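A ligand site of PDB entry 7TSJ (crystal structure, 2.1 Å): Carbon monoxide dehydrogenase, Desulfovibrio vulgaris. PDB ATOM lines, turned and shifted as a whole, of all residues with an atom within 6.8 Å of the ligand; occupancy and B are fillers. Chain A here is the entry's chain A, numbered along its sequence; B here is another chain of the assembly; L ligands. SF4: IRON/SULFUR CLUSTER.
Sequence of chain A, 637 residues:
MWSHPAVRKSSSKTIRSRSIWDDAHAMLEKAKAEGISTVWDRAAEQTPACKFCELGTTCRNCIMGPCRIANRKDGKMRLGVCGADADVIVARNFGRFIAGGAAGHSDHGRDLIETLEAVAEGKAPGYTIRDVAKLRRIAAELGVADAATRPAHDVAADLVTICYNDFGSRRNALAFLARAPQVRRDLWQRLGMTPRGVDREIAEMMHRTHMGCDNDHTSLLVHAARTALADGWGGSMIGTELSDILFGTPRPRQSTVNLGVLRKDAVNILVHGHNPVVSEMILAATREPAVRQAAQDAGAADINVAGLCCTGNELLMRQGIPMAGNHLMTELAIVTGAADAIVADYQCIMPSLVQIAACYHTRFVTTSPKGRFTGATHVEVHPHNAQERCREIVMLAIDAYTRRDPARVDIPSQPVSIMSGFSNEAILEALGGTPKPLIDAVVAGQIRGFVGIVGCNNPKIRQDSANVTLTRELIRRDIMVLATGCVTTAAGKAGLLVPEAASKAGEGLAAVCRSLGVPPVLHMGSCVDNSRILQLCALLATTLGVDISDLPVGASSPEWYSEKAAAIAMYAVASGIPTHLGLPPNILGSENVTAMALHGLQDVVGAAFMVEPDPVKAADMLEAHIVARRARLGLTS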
ATOM      1  N   THR A  58       8.673 -26.043 -16.679  1.00  0.00           N
ATOM      2  CA  THR A  58       8.165 -27.320 -16.205  1.00  0.00           C
ATOM      3  C   THR A  58       7.302 -27.048 -14.980  1.00  0.00           C
ATOM      4  O   THR A  58       7.593 -26.158 -14.184  1.00  0.00           O
ATOM      5  CB  THR A  58       9.295 -28.275 -15.837  1.00  0.00           C
ATOM      6  OG1 THR A  58       8.745 -29.527 -15.424  1.00  0.00           O
ATOM      7  CG2 THR A  58      10.139 -27.710 -14.707  1.00  0.00           C
ATOM      8  N   CYS A  59       6.211 -27.794 -14.861  1.00  0.00           N
ATOM      9  CA  CYS A  59       5.268 -27.606 -13.770  1.00  0.00           C
ATOM     10  C   CYS A  59       4.876 -28.949 -13.175  1.00  0.00           C
ATOM     11  O   CYS A  59       4.667 -29.917 -13.909  1.00  0.00           O
ATOM     12  CB  CYS A  59       4.029 -26.853 -14.233  1.00  0.00           C
ATOM     13  SG  CYS A  59       3.060 -26.260 -12.871  1.00  0.00           S
ATOM     14  N   ARG A  60       4.826 -29.002 -11.833  1.00  0.00           N
ATOM     15  CA  ARG A  60       4.400 -30.182 -11.080  1.00  0.00           C
ATOM     16  C   ARG A  60       3.436 -29.789  -9.967  1.00  0.00           C
ATOM     17  O   ARG A  60       3.386 -30.428  -8.916  1.00  0.00           O
ATOM     18  CB  ARG A  60       5.609 -30.919 -10.501  1.00  0.00           C
ATOM     19  CG  ARG A  60       6.851 -30.937 -11.391  1.00  0.00           C
ATOM     20  CD  ARG A  60       8.022 -31.646 -10.694  1.00  0.00           C
ATOM     21  NE  ARG A  60       7.958 -31.435  -9.251  1.00  0.00           N
ATOM     22  CZ  ARG A  60       8.811 -30.684  -8.559  1.00  0.00           C
ATOM     23  NH1 ARG A  60       9.888 -30.155  -9.117  1.00  0.00           N
ATOM     24  NH2 ARG A  60       8.575 -30.468  -7.261  1.00  0.00           N
ATOM     25  N   ASN A  61       2.683 -28.712 -10.183  1.00  0.00           N
ATOM     26  CA  ASN A  61       1.780 -28.181  -9.172  1.00  0.00           C
ATOM     27  C   ASN A  61       0.458 -28.937  -9.086  1.00  0.00           C
ATOM     28  O   ASN A  61      -0.331 -28.664  -8.174  1.00  0.00           O
ATOM     29  CB  ASN A  61       1.504 -26.690  -9.435  1.00  0.00           C
ATOM     30  CG  ASN A  61       2.712 -25.818  -9.099  1.00  0.00           C
ATOM     31  OD1 ASN A  61       3.811 -26.335  -8.855  1.00  0.00           O
ATOM     32  ND2 ASN A  61       2.518 -24.503  -9.093  1.00  0.00           N
ATOM     33  N   CYS A  62       0.197 -29.888  -9.969  1.00  0.00           N
ATOM     34  CA  CYS A  62      -0.918 -30.814  -9.769  1.00  0.00           C
ATOM     35  C   CYS A  62      -0.615 -32.069 -10.557  1.00  0.00           C
ATOM     36  O   CYS A  62       0.330 -32.100 -11.353  1.00  0.00           O
ATOM     37  CB  CYS A  62      -2.255 -30.186 -10.179  1.00  0.00           C
ATOM     38  SG  CYS A  62      -2.644 -30.303 -11.938  1.00  0.00           S
ATOM     39  N   ILE A  63      -1.392 -33.120 -10.326  1.00  0.00           N
ATOM     40  CA  ILE A  63      -1.174 -34.407 -10.992  1.00  0.00           C
ATOM     41  C   ILE A  63      -2.117 -34.587 -12.190  1.00  0.00           C
ATOM     42  O   ILE A  63      -2.281 -35.700 -12.679  1.00  0.00           O
ATOM     43  CB  ILE A  63      -1.279 -35.586 -10.018  1.00  0.00           C
ATOM     44  CG1 ILE A  63      -2.734 -35.761  -9.531  1.00  0.00           C
ATOM     45  CG2 ILE A  63      -0.307 -35.434  -8.853  1.00  0.00           C
ATOM     46  CD1 ILE A  63      -3.052 -37.175  -9.073  1.00  0.00           C
ATOM     47  N   MET A  64      -2.718 -33.509 -12.696  1.00  0.00           N
ATOM     48  CA  MET A  64      -3.069 -33.546 -14.107  1.00  0.00           C
ATOM     49  C   MET A  64      -1.801 -33.599 -14.937  1.00  0.00           C
ATOM     50  O   MET A  64      -1.738 -34.308 -15.937  1.00  0.00           O
ATOM     51  CB  MET A  64      -3.910 -32.339 -14.498  1.00  0.00           C
ATOM     52  CG  MET A  64      -5.321 -32.392 -13.957  1.00  0.00           C
ATOM     53  SD  MET A  64      -6.440 -31.410 -14.963  1.00  0.00           S
ATOM     54  CE  MET A  64      -5.920 -29.762 -14.513  1.00  0.00           C
ATOM     55  N   GLY A  65      -0.768 -32.886 -14.497  1.00  0.00           N
ATOM     56  CA  GLY A  65       0.551 -33.034 -15.076  1.00  0.00           C
ATOM     57  C   GLY A  65       1.290 -34.231 -14.506  1.00  0.00           C
ATOM     58  O   GLY A  65       0.673 -35.245 -14.139  1.00  0.00           O
ATOM     59  N   PRO A  66       2.630 -34.122 -14.362  1.00  0.00           N
ATOM     60  CA  PRO A  66       3.470 -32.924 -14.521  1.00  0.00           C
ATOM     61  C   PRO A  66       3.614 -32.495 -15.979  1.00  0.00           C
ATOM     62  O   PRO A  66       3.485 -33.307 -16.882  1.00  0.00           O
ATOM     63  CB  PRO A  66       4.800 -33.363 -13.905  1.00  0.00           C
ATOM     64  CG  PRO A  66       4.866 -34.830 -14.213  1.00  0.00           C
ATOM     65  CD  PRO A  66       3.437 -35.300 -14.017  1.00  0.00           C
ATOM     66  N   CYS A  67       3.880 -31.211 -16.220  1.00  0.00           N
ATOM     67  CA  CYS A  67       3.856 -30.640 -17.554  1.00  0.00           C
ATOM     68  C   CYS A  67       5.191 -30.012 -17.907  1.00  0.00           C
ATOM     69  O   CYS A  67       5.930 -29.545 -17.029  1.00  0.00           O
ATOM     70  CB  CYS A  67       2.749 -29.600 -17.673  1.00  0.00           C
ATOM     71  SG  CYS A  67       1.083 -30.309 -17.465  1.00  0.00           S
ATOM     72  N   ARG A  68       5.481 -29.989 -19.200  1.00  0.00           N
ATOM     73  CA  ARG A  68       6.622 -29.264 -19.742  1.00  0.00           C
ATOM     74  C   ARG A  68       6.149 -28.455 -20.935  1.00  0.00           C
ATOM     75  O   ARG A  68       5.305 -28.913 -21.714  1.00  0.00           O
ATOM     76  CB  ARG A  68       7.731 -30.213 -20.181  1.00  0.00           C
ATOM     77  CG  ARG A  68       8.440 -30.899 -19.053  1.00  0.00           C
ATOM     78  CD  ARG A  68       9.099 -32.141 -19.577  1.00  0.00           C
ATOM     79  NE  ARG A  68       8.103 -33.165 -19.846  1.00  0.00           N
ATOM     80  CZ  ARG A  68       8.244 -34.092 -20.783  1.00  0.00           C
ATOM     81  NH1 ARG A  68       9.322 -34.144 -21.545  1.00  0.00           N
ATOM     82  NH2 ARG A  68       7.259 -34.982 -20.968  1.00  0.00           N
ATOM     83  N   ILE A  69       6.690 -27.251 -21.090  1.00  0.00           N
ATOM     84  CA  ILE A  69       6.316 -26.368 -22.185  1.00  0.00           C
ATOM     85  C   ILE A  69       7.435 -26.388 -23.206  1.00  0.00           C
ATOM     86  O   ILE A  69       8.604 -26.204 -22.868  1.00  0.00           O
ATOM     87  CB  ILE A  69       6.061 -24.943 -21.679  1.00  0.00           C
ATOM     88  CG1 ILE A  69       4.929 -24.964 -20.650  1.00  0.00           C
ATOM     89  CG2 ILE A  69       5.716 -24.018 -22.838  1.00  0.00           C
ATOM     90  CD1 ILE A  69       3.639 -25.542 -21.203  1.00  0.00           C
ATOM     91  N   LEU A  79       1.159 -25.674 -24.040  1.00  0.00           N
ATOM     92  CA  LEU A  79       0.326 -25.317 -22.909  1.00  0.00           C
ATOM     93  C   LEU A  79       0.300 -26.458 -21.901  1.00  0.00           C
ATOM     94  O   LEU A  79       0.362 -27.635 -22.260  1.00  0.00           O
ATOM     95  CB  LEU A  79      -1.109 -25.008 -23.346  1.00  0.00           C
ATOM     96  CG  LEU A  79      -1.344 -23.786 -24.218  1.00  0.00           C
ATOM     97  CD1 LEU A  79      -2.813 -23.758 -24.638  1.00  0.00           C
ATOM     98  CD2 LEU A  79      -0.970 -22.536 -23.456  1.00  0.00           C
ATOM     99  N   GLY A  80       0.197 -26.084 -20.621  1.00  0.00           N
ATOM    100  CA  GLY A  80      -0.095 -27.072 -19.602  1.00  0.00           C
ATOM    101  C   GLY A  80      -1.469 -27.701 -19.813  1.00  0.00           C
ATOM    102  O   GLY A  80      -2.300 -27.212 -20.571  1.00  0.00           O
ATOM    103  N   VAL A  81      -1.691 -28.827 -19.120  1.00  0.00           N
ATOM    104  CA  VAL A  81      -2.968 -29.515 -19.288  1.00  0.00           C
ATOM    105  C   VAL A  81      -4.100 -28.584 -18.874  1.00  0.00           C
ATOM    106  O   VAL A  81      -5.136 -28.511 -19.551  1.00  0.00           O
ATOM    107  CB  VAL A  81      -2.987 -30.827 -18.483  1.00  0.00           C
ATOM    108  CG1 VAL A  81      -4.366 -31.472 -18.546  1.00  0.00           C
ATOM    109  CG2 VAL A  81      -1.932 -31.783 -19.031  1.00  0.00           C
ATOM    110  N   CYS A  82      -3.890 -27.822 -17.812  1.00  0.00           N
ATOM    111  CA  CYS A  82      -4.834 -26.799 -17.374  1.00  0.00           C
ATOM    112  C   CYS A  82      -4.908 -25.607 -18.334  1.00  0.00           C
ATOM    113  O   CYS A  82      -5.711 -24.709 -18.083  1.00  0.00           O
ATOM    114  CB  CYS A  82      -4.454 -26.305 -15.983  1.00  0.00           C
ATOM    115  SG  CYS A  82      -2.991 -25.189 -16.001  1.00  0.00           S
ATOM    116  N   GLY A  83      -4.129 -25.579 -19.410  1.00  0.00           N
ATOM    117  CA  GLY A  83      -4.055 -24.420 -20.294  1.00  0.00           C
ATOM    118  C   GLY A  83      -2.988 -23.390 -19.959  1.00  0.00           C
ATOM    119  O   GLY A  83      -2.818 -22.431 -20.720  1.00  0.00           O
ATOM    120  N   ALA A  84      -2.260 -23.535 -18.861  1.00  0.00           N
ATOM    121  CA  ALA A  84      -1.236 -22.557 -18.498  1.00  0.00           C
ATOM    122  C   ALA A  84      -0.089 -22.545 -19.514  1.00  0.00           C
ATOM    123  O   ALA A  84       0.374 -23.606 -19.950  1.00  0.00           O
ATOM    124  CB  ALA A  84      -0.678 -22.857 -17.118  1.00  0.00           C
ATOM    125  N   ASP A  85       0.375 -21.332 -19.877  1.00  0.00           N
ATOM    126  CA  ASP A  85       1.458 -21.167 -20.843  1.00  0.00           C
ATOM    127  C   ASP A  85       2.803 -20.952 -20.141  1.00  0.00           C
ATOM    128  O   ASP A  85       2.910 -20.894 -18.917  1.00  0.00           O
ATOM    129  CB  ASP A  85       1.143 -20.030 -21.836  1.00  0.00           C
ATOM    130  CG  ASP A  85       1.001 -18.655 -21.157  1.00  0.00           C
ATOM    131  OD1 ASP A  85       1.362 -18.493 -19.964  1.00  0.00           O
ATOM    132  OD2 ASP A  85       0.545 -17.709 -21.844  1.00  0.00           O
ATOM    133  N   ILE A  89       3.713 -20.443 -16.068  1.00  0.00           N
ATOM    134  CA  ILE A  89       4.441 -21.495 -15.356  1.00  0.00           C
ATOM    135  C   ILE A  89       5.777 -20.976 -14.832  1.00  0.00           C
ATOM    136  O   ILE A  89       6.135 -21.226 -13.676  1.00  0.00           O
ATOM    137  CB  ILE A  89       4.625 -22.718 -16.270  1.00  0.00           C
ATOM    138  CG1 ILE A  89       3.299 -23.470 -16.406  1.00  0.00           C
ATOM    139  CG2 ILE A  89       5.690 -23.629 -15.704  1.00  0.00           C
ATOM    140  CD1 ILE A  89       3.271 -24.403 -17.568  1.00  0.00           C
ATOM    141  N   ARG A  92       5.191 -18.673 -11.920  1.00  0.00           N
ATOM    142  CA  ARG A  92       4.776 -19.380 -10.706  1.00  0.00           C
ATOM    143  C   ARG A  92       5.964 -20.051 -10.040  1.00  0.00           C
ATOM    144  O   ARG A  92       6.130 -19.976  -8.827  1.00  0.00           O
ATOM    145  CB  ARG A  92       3.684 -20.411 -11.013  1.00  0.00           C
ATOM    146  CG  ARG A  92       2.341 -19.776 -11.266  1.00  0.00           C
ATOM    147  CD  ARG A  92       1.196 -20.806 -11.252  1.00  0.00           C
ATOM    148  NE  ARG A  92       1.476 -21.914 -12.148  1.00  0.00           N
ATOM    149  CZ  ARG A  92       0.546 -22.648 -12.732  1.00  0.00           C
ATOM    150  NH1 ARG A  92      -0.738 -22.384 -12.572  1.00  0.00           N
ATOM    151  NH2 ARG A  92       0.918 -23.673 -13.501  1.00  0.00           N
ATOM    152  N   THR A 209      -0.083 -19.655  -6.587  1.00  0.00           N
ATOM    153  CA  THR A 209       0.582 -20.562  -7.520  1.00  0.00           C
ATOM    154  C   THR A 209      -0.049 -21.943  -7.569  1.00  0.00           C
ATOM    155  O   THR A 209       0.355 -22.762  -8.408  1.00  0.00           O
ATOM    156  CB  THR A 209       2.087 -20.664  -7.189  1.00  0.00           C
ATOM    157  OG1 THR A 209       2.268 -21.126  -5.845  1.00  0.00           O
ATOM    158  CG2 THR A 209       2.731 -19.278  -7.303  1.00  0.00           C
ATOM    159  N   HIS A 210      -1.044 -22.231  -6.712  1.00  0.00           N
ATOM    160  CA  HIS A 210      -1.908 -23.384  -6.926  1.00  0.00           C
ATOM    161  C   HIS A 210      -2.568 -23.255  -8.304  1.00  0.00           C
ATOM    162  O   HIS A 210      -2.808 -22.149  -8.807  1.00  0.00           O
ATOM    163  CB  HIS A 210      -2.966 -23.474  -5.805  1.00  0.00           C
ATOM    164  CG  HIS A 210      -3.789 -24.739  -5.813  1.00  0.00           C
ATOM    165  ND1 HIS A 210      -4.716 -25.029  -6.791  1.00  0.00           N
ATOM    166  CD2 HIS A 210      -3.855 -25.764  -4.924  1.00  0.00           C
ATOM    167  CE1 HIS A 210      -5.285 -26.197  -6.530  1.00  0.00           C
ATOM    168  NE2 HIS A 210      -4.784 -26.667  -5.396  1.00  0.00           N
ATOM    169  N   MET A 211      -2.842 -24.395  -8.928  1.00  0.00           N
ATOM    170  CA  MET A 211      -3.438 -24.350 -10.259  1.00  0.00           C
ATOM    171  C   MET A 211      -4.775 -23.628 -10.221  1.00  0.00           C
ATOM    172  O   MET A 211      -5.526 -23.693  -9.235  1.00  0.00           O
ATOM    173  CB  MET A 211      -3.593 -25.765 -10.828  1.00  0.00           C
ATOM    174  CG  MET A 211      -4.999 -26.182 -11.181  1.00  0.00           C
ATOM    175  SD  MET A 211      -5.842 -25.409 -12.592  1.00  0.00           S
ATOM    176  CE  MET A 211      -7.259 -26.477 -12.624  1.00  0.00           C
ATOM    177  N   GLY A 212      -5.056 -22.899 -11.300  1.00  0.00           N
ATOM    178  CA  GLY A 212      -6.313 -22.193 -11.420  1.00  0.00           C
ATOM    179  C   GLY A 212      -6.502 -21.082 -10.421  1.00  0.00           C
ATOM    180  O   GLY A 212      -7.632 -20.834  -9.990  1.00  0.00           O
ATOM    181  N   GLN B  46       0.787 -33.935 -23.223  1.00  0.00           N
ATOM    182  CA  GLN B  46       1.746 -34.041 -22.137  1.00  0.00           C
ATOM    183  C   GLN B  46       1.992 -35.481 -21.716  1.00  0.00           C
ATOM    184  O   GLN B  46       2.432 -35.731 -20.588  1.00  0.00           O
ATOM    185  CB  GLN B  46       1.272 -33.219 -20.934  1.00  0.00           C
ATOM    186  CG  GLN B  46       1.231 -31.719 -21.200  1.00  0.00           C
ATOM    187  CD  GLN B  46       2.624 -31.092 -21.310  1.00  0.00           C
ATOM    188  OE1 GLN B  46       3.623 -31.718 -20.961  1.00  0.00           O
ATOM    189  NE2 GLN B  46       2.690 -29.861 -21.797  1.00  0.00           N
ATOM    190  N   PRO B 351      -7.141 -21.856 -16.742  1.00  0.00           N
ATOM    191  CA  PRO B 351      -6.928 -20.702 -17.625  1.00  0.00           C
ATOM    192  C   PRO B 351      -7.397 -20.941 -19.045  1.00  0.00           C
ATOM    193  O   PRO B 351      -7.616 -19.965 -19.774  1.00  0.00           O
ATOM    194  CB  PRO B 351      -5.414 -20.480 -17.555  1.00  0.00           C
ATOM    195  CG  PRO B 351      -4.848 -21.786 -17.067  1.00  0.00           C
ATOM    196  CD  PRO B 351      -5.882 -22.333 -16.133  1.00  0.00           C
ATOM    197  N   TYR B 561      -6.840 -34.398  -8.416  1.00  0.00           N
ATOM    198  CA  TYR B 561      -5.750 -33.795  -9.170  1.00  0.00           C
ATOM    199  C   TYR B 561      -4.992 -32.708  -8.410  1.00  0.00           C
ATOM    200  O   TYR B 561      -3.810 -32.508  -8.692  1.00  0.00           O
ATOM    201  CB  TYR B 561      -6.258 -33.211 -10.524  1.00  0.00           C
ATOM    202  CG  TYR B 561      -6.706 -31.785 -10.399  1.00  0.00           C
ATOM    203  CD1 TYR B 561      -5.778 -30.741 -10.493  1.00  0.00           C
ATOM    204  CD2 TYR B 561      -8.029 -31.467 -10.139  1.00  0.00           C
ATOM    205  CE1 TYR B 561      -6.157 -29.428 -10.326  1.00  0.00           C
ATOM    206  CE2 TYR B 561      -8.431 -30.132  -9.984  1.00  0.00           C
ATOM    207  CZ  TYR B 561      -7.473 -29.123 -10.068  1.00  0.00           C
ATOM    208  OH  TYR B 561      -7.802 -27.797  -9.913  1.00  0.00           O
HETATM  209 FE1  SF4 L   1       0.997 -27.260 -13.696  1.00  0.00          FE
HETATM  210 FE2  SF4 L   1       0.285 -28.969 -15.637  1.00  0.00          FE
HETATM  211 FE3  SF4 L   1      -1.352 -26.886 -14.981  1.00  0.00          FE
HETATM  212 FE4  SF4 L   1      -1.027 -28.955 -13.241  1.00  0.00          FE
HETATM  213  S1  SF4 L   1      -1.943 -29.037 -15.297  1.00  0.00           S
HETATM  214  S2  SF4 L   1      -0.998 -26.724 -12.730  1.00  0.00           S
HETATM  215  S3  SF4 L   1       1.170 -29.527 -13.595  1.00  0.00           S
HETATM  216  S4  SF4 L   1       0.764 -26.749 -15.863  1.00  0.00           S
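Residues that only touch the ligand: Asn 61, Met 64, Gly 65, Gly 80, Val 81, Ile 89 and Met 211. Hydrophobic or aromatic side chains that line the ligand: Met 64, Val 81, Ile 89 and Met 211. 12 residues have an atom within 4 Å of the ligand: Cys 59, Asn 61, Cys 62, Met 64, Gly 65, Cys 67, Gly 80, Val 81, Cys 82, Ile 89, Arg 92 and Met 211. The nearest printed residue that does not touch the ligand is Arg 60 (4.1 Å).
The backbone carbonyl oxygen (O) of Cys 59 lies within hydrogen-bond range of the backbone NH (N) of Cys 67, 2.8 Å away. N of Val 81 lies close to SG of Cys 67 (3.6 Å). The backbone carbonyl oxygen (O) of Cys 67 sits at hydrogen-bond distance from the side-chain hydroxyl (OG1) of Thr 58, at 3.2 Å. The side-chain sulfur (SG) of Cys 59 sits close to the guanidinium group (NH2) of Arg 92. The side-chain sulfur (SG) of Cys 59 sits close to the backbone NH (N) of Asn 61. The side-chain sulfur of Cys 62 sits close to the backbone NH of Met 64, at 3.3 Å. SG of Cys 82 lies close to N of Ala 84 (3.4 Å). The side-chain amide nitrogen (ND2) of Asn 61 lies within hydrogen-bond range of the backbone carbonyl oxygen (O) of Thr 209, at 2.9 Å.
SG of Cys 67 binds FE2 of the ligand, 2.4 Å away. The side-chain sulfur (SG) of Cys 59 is bound to an iron atom (FE1) of the ligand, at 2.4 Å. N of Cys 62 lies close to S3 of the ligand (3.8 Å). The side-chain sulfur (SG) of Cys 62 binds an iron atom (FE4) of the ligand, 2.5 Å away. S1 of the ligand sits close to N of Cys 82. The side-chain sulfur of Cys 82 binds an iron atom (FE3) of the ligand, at 2.6 Å. The guanidinium group (NH2) of Arg 92 sits close to a sulfur (S2) of the ligand (3.7 Å).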
